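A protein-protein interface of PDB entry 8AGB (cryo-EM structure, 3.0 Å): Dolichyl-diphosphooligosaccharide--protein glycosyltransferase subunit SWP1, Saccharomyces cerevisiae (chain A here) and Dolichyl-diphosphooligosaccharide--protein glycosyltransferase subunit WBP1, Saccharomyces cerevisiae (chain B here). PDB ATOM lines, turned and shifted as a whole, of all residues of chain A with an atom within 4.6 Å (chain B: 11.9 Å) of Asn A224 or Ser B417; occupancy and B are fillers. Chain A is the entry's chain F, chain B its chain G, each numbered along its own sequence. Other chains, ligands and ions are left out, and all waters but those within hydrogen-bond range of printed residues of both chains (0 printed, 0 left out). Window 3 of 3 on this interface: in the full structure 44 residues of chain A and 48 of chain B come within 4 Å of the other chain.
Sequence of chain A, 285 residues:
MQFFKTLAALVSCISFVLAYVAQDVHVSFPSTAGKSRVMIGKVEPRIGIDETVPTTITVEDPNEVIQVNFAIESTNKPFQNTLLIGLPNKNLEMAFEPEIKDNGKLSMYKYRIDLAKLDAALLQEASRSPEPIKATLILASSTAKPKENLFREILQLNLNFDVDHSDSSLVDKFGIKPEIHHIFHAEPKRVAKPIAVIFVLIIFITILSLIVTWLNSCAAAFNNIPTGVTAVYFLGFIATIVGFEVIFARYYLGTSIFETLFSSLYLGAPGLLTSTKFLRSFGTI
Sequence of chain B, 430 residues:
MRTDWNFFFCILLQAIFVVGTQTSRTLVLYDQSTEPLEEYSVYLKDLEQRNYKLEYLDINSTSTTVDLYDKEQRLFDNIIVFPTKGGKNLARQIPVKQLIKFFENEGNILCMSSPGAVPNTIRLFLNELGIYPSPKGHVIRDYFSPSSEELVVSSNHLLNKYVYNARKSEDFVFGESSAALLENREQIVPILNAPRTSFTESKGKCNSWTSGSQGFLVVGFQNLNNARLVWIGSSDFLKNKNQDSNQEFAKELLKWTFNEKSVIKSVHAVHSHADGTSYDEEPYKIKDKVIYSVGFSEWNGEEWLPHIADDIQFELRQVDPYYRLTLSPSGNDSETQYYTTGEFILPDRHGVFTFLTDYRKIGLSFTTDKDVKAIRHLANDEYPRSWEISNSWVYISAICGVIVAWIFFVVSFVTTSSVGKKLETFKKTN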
ATOM      1  N   ASN A 223     -20.050  17.957   5.352  1.00  0.00           N
ATOM      2  CA  ASN A 223     -20.050  16.525   5.104  1.00  0.00           C
ATOM      3  C   ASN A 223     -20.685  15.868   6.326  1.00  0.00           C
ATOM      4  O   ASN A 223     -21.197  16.557   7.212  1.00  0.00           O
ATOM      5  CB  ASN A 223     -18.636  16.011   4.827  1.00  0.00           C
ATOM      6  CG  ASN A 223     -17.661  16.366   5.926  1.00  0.00           C
ATOM      7  OD1 ASN A 223     -17.581  15.681   6.945  1.00  0.00           O
ATOM      8  ND2 ASN A 223     -16.913  17.443   5.726  1.00  0.00           N
ATOM      9  N   ASN A 224     -20.620  14.537   6.388  1.00  0.00           N
ATOM     10  CA  ASN A 224     -21.128  13.783   7.532  1.00  0.00           C
ATOM     11  C   ASN A 224     -22.465  14.316   8.038  1.00  0.00           C
ATOM     12  O   ASN A 224     -22.670  14.450   9.248  1.00  0.00           O
ATOM     13  CB  ASN A 224     -20.100  13.800   8.665  1.00  0.00           C
ATOM     14  CG  ASN A 224     -20.303  12.671   9.652  1.00  0.00           C
ATOM     15  OD1 ASN A 224     -20.533  12.903  10.838  1.00  0.00           O
ATOM     16  ND2 ASN A 224     -20.222  11.436   9.167  1.00  0.00           N
ATOM     17  N   ILE A 225     -23.375  14.628   7.119  1.00  0.00           N
ATOM     18  CA  ILE A 225     -24.726  15.059   7.470  1.00  0.00           C
ATOM     19  C   ILE A 225     -25.587  13.823   7.695  1.00  0.00           C
ATOM     20  O   ILE A 225     -25.694  12.973   6.800  1.00  0.00           O
ATOM     21  CB  ILE A 225     -25.337  15.959   6.384  1.00  0.00           C
ATOM     22  CG1 ILE A 225     -24.525  17.244   6.228  1.00  0.00           C
ATOM     23  CG2 ILE A 225     -26.784  16.282   6.717  1.00  0.00           C
ATOM     24  CD1 ILE A 225     -25.254  18.340   5.477  1.00  0.00           C
ATOM     25  N   PRO A 226     -26.210  13.681   8.862  1.00  0.00           N
ATOM     26  CA  PRO A 226     -27.096  12.533   9.082  1.00  0.00           C
ATOM     27  C   PRO A 226     -28.330  12.609   8.197  1.00  0.00           C
ATOM     28  O   PRO A 226     -28.913  13.677   7.999  1.00  0.00           O
ATOM     29  CB  PRO A 226     -27.461  12.652  10.565  1.00  0.00           C
ATOM     30  CG  PRO A 226     -27.340  14.107  10.854  1.00  0.00           C
ATOM     31  CD  PRO A 226     -26.204  14.605  10.008  1.00  0.00           C
ATOM     32  N   PHE A 282     -25.773  10.464  17.758  1.00  0.00           N
ATOM     33  CA  PHE A 282     -24.584  10.906  17.036  1.00  0.00           C
ATOM     34  C   PHE A 282     -23.359  10.617  17.897  1.00  0.00           C
ATOM     35  O   PHE A 282     -23.133  11.280  18.914  1.00  0.00           O
ATOM     36  CB  PHE A 282     -24.695  12.387  16.677  1.00  0.00           C
ATOM     37  CG  PHE A 282     -23.374  13.067  16.440  1.00  0.00           C
ATOM     38  CD1 PHE A 282     -22.788  13.040  15.186  1.00  0.00           C
ATOM     39  CD2 PHE A 282     -22.744  13.779  17.450  1.00  0.00           C
ATOM     40  CE1 PHE A 282     -21.580  13.671  14.953  1.00  0.00           C
ATOM     41  CE2 PHE A 282     -21.538  14.410  17.224  1.00  0.00           C
ATOM     42  CZ  PHE A 282     -20.957  14.359  15.973  1.00  0.00           C
ATOM     43  N   PHE B 409     -21.825  28.390  13.871  1.00  0.00           N
ATOM     44  CA  PHE B 409     -20.733  27.577  14.385  1.00  0.00           C
ATOM     45  C   PHE B 409     -21.238  26.298  15.023  1.00  0.00           C
ATOM     46  O   PHE B 409     -20.609  25.251  14.871  1.00  0.00           O
ATOM     47  CB  PHE B 409     -19.909  28.379  15.389  1.00  0.00           C
ATOM     48  CG  PHE B 409     -19.064  27.533  16.292  1.00  0.00           C
ATOM     49  CD1 PHE B 409     -17.873  26.998  15.842  1.00  0.00           C
ATOM     50  CD2 PHE B 409     -19.452  27.284  17.595  1.00  0.00           C
ATOM     51  CE1 PHE B 409     -17.094  26.224  16.668  1.00  0.00           C
ATOM     52  CE2 PHE B 409     -18.674  26.509  18.425  1.00  0.00           C
ATOM     53  CZ  PHE B 409     -17.494  25.978  17.961  1.00  0.00           C
ATOM     54  N   VAL B 410     -22.338  26.357  15.771  1.00  0.00           N
ATOM     55  CA  VAL B 410     -22.878  25.132  16.357  1.00  0.00           C
ATOM     56  C   VAL B 410     -23.237  24.141  15.256  1.00  0.00           C
ATOM     57  O   VAL B 410     -22.897  22.951  15.322  1.00  0.00           O
ATOM     58  CB  VAL B 410     -24.087  25.446  17.252  1.00  0.00           C
ATOM     59  CG1 VAL B 410     -24.770  24.164  17.677  1.00  0.00           C
ATOM     60  CG2 VAL B 410     -23.646  26.238  18.462  1.00  0.00           C
ATOM     61  N   VAL B 411     -23.933  24.626  14.225  1.00  0.00           N
ATOM     62  CA  VAL B 411     -24.342  23.780  13.107  1.00  0.00           C
ATOM     63  C   VAL B 411     -23.127  23.186  12.404  1.00  0.00           C
ATOM     64  O   VAL B 411     -23.086  21.986  12.109  1.00  0.00           O
ATOM     65  CB  VAL B 411     -25.212  24.581  12.124  1.00  0.00           C
ATOM     66  CG1 VAL B 411     -25.594  23.723  10.931  1.00  0.00           C
ATOM     67  CG2 VAL B 411     -26.435  25.124  12.823  1.00  0.00           C
ATOM     68  N   SER B 412     -22.121  24.013  12.117  1.00  0.00           N
ATOM     69  CA  SER B 412     -20.953  23.483  11.427  1.00  0.00           C
ATOM     70  C   SER B 412     -20.063  22.634  12.326  1.00  0.00           C
ATOM     71  O   SER B 412     -19.243  21.871  11.817  1.00  0.00           O
ATOM     72  CB  SER B 412     -20.139  24.625  10.821  1.00  0.00           C
ATOM     73  OG  SER B 412     -20.071  25.727  11.707  1.00  0.00           O
ATOM     74  N   PHE B 413     -20.182  22.757  13.645  1.00  0.00           N
ATOM     75  CA  PHE B 413     -19.454  21.858  14.531  1.00  0.00           C
ATOM     76  C   PHE B 413     -20.110  20.487  14.623  1.00  0.00           C
ATOM     77  O   PHE B 413     -19.413  19.470  14.688  1.00  0.00           O
ATOM     78  CB  PHE B 413     -19.335  22.487  15.919  1.00  0.00           C
ATOM     79  CG  PHE B 413     -18.460  21.718  16.863  1.00  0.00           C
ATOM     80  CD1 PHE B 413     -18.975  20.706  17.649  1.00  0.00           C
ATOM     81  CD2 PHE B 413     -17.117  22.026  16.976  1.00  0.00           C
ATOM     82  CE1 PHE B 413     -18.166  20.008  18.518  1.00  0.00           C
ATOM     83  CE2 PHE B 413     -16.305  21.333  17.844  1.00  0.00           C
ATOM     84  CZ  PHE B 413     -16.831  20.323  18.616  1.00  0.00           C
ATOM     85  N   VAL B 414     -21.443  20.432  14.628  1.00  0.00           N
ATOM     86  CA  VAL B 414     -22.107  19.129  14.663  1.00  0.00           C
ATOM     87  C   VAL B 414     -22.037  18.437  13.306  1.00  0.00           C
ATOM     88  O   VAL B 414     -21.668  17.261  13.219  1.00  0.00           O
ATOM     89  CB  VAL B 414     -23.562  19.248  15.162  1.00  0.00           C
ATOM     90  CG1 VAL B 414     -23.588  19.433  16.669  1.00  0.00           C
ATOM     91  CG2 VAL B 414     -24.311  20.356  14.459  1.00  0.00           C
ATOM     92  N   THR B 415     -22.409  19.145  12.237  1.00  0.00           N
ATOM     93  CA  THR B 415     -22.494  18.528  10.914  1.00  0.00           C
ATOM     94  C   THR B 415     -21.181  17.869  10.500  1.00  0.00           C
ATOM     95  O   THR B 415     -21.160  16.690  10.133  1.00  0.00           O
ATOM     96  CB  THR B 415     -22.921  19.575   9.886  1.00  0.00           C
ATOM     97  OG1 THR B 415     -24.348  19.694   9.897  1.00  0.00           O
ATOM     98  CG2 THR B 415     -22.473  19.174   8.495  1.00  0.00           C
ATOM     99  N   THR B 416     -20.077  18.607  10.554  1.00  0.00           N
ATOM    100  CA  THR B 416     -18.825  18.097  10.012  1.00  0.00           C
ATOM    101  C   THR B 416     -18.153  17.128  10.976  1.00  0.00           C
ATOM    102  O   THR B 416     -18.272  17.244  12.199  1.00  0.00           O
ATOM    103  CB  THR B 416     -17.866  19.240   9.689  1.00  0.00           C
ATOM    104  OG1 THR B 416     -17.074  19.546  10.843  1.00  0.00           O
ATOM    105  CG2 THR B 416     -18.641  20.467   9.265  1.00  0.00           C
ATOM    106  N   SER B 417     -17.440  16.162  10.404  1.00  0.00           N
ATOM    107  CA  SER B 417     -16.713  15.155  11.160  1.00  0.00           C
ATOM    108  C   SER B 417     -15.224  15.475  11.173  1.00  0.00           C
ATOM    109  O   SER B 417     -14.705  16.147  10.278  1.00  0.00           O
ATOM    110  CB  SER B 417     -16.937  13.762  10.569  1.00  0.00           C
ATOM    111  OG  SER B 417     -15.863  12.896  10.896  1.00  0.00           O
ATOM    112  N   SER B 418     -14.539  14.982  12.199  1.00  0.00           N
ATOM    113  CA  SER B 418     -13.106  15.209  12.339  1.00  0.00           C
ATOM    114  C   SER B 418     -12.307  14.218  11.499  1.00  0.00           C
ATOM    115  O   SER B 418     -11.077  14.267  11.466  1.00  0.00           O
ATOM    116  CB  SER B 418     -12.690  15.110  13.808  1.00  0.00           C
ATOM    117  OG  SER B 418     -13.391  14.069  14.465  1.00  0.00           O
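O of Asn A223 sits close to O of Thr B415 (2.9 Å).
The backbone carbonyl oxygen (O) of Asn A224 lies close to the backbone carbonyl oxygen (O) of Thr B415 (2.8 Å).
The backbone NH of Ser B417 sits at hydrogen-bond distance from the side-chain amide oxygen of Asn A223.
The side-chain hydroxyl of Thr B416 sits close to the backbone carbonyl oxygen of Ser B412 (3.3 Å).
The side-chain hydroxyl (OG1) of Thr B415 lies close to the backbone carbonyl oxygen (O) of Val B411 (3.4 Å).
Among the printed residues, pairs that only touch across the chains: Ile A225 with Thr B415 (3.6 Å), Asn A224 with Ser B417 (3.7 Å), Asn A223 with Thr B416 (3.98 Å) and Phe A282 with Val B414 (3.99 Å).
Asn A224 touches just these residues of chain B: Thr B415 and Ser B417.
Ser B417 touches just these residues of chain A: Asn A223 and Asn A224.
Printed residues of chain B within 4 Å of Asn A223: Thr B415 (2.9 Å), Thr B416 (3.98 Å) and Ser B417 (3.5 Å).
Of the printed residues of chain B, Ile A225 touches Thr B415 (3.6 Å).
No residue of chain B comes within 4 Å of Pro A226.
Printed residues of chain A within 4 Å of Thr B415: Asn A223 (2.9 Å), Asn A224 (2.8 Å) and Ile A225 (3.6 Å).
Printed residues of chain B within 4 Å of Phe A282: Val B414.
Of the printed residues of chain A, Thr B416 touches Asn A223.
Printed residues of chain A within 4 Å of Val B414: Phe A282.
The nearest residue of chain B that does not touch Asn A224 is Thr B416 (4.5 Å).
The nearest printed residue of chain A that does not touch Thr B416 is Asn A224 (4.5 Å).
Hydrophobic or aromatic side chains of chain A within 4 Å of the printed part of chain B: Ile A225 and Phe A282.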
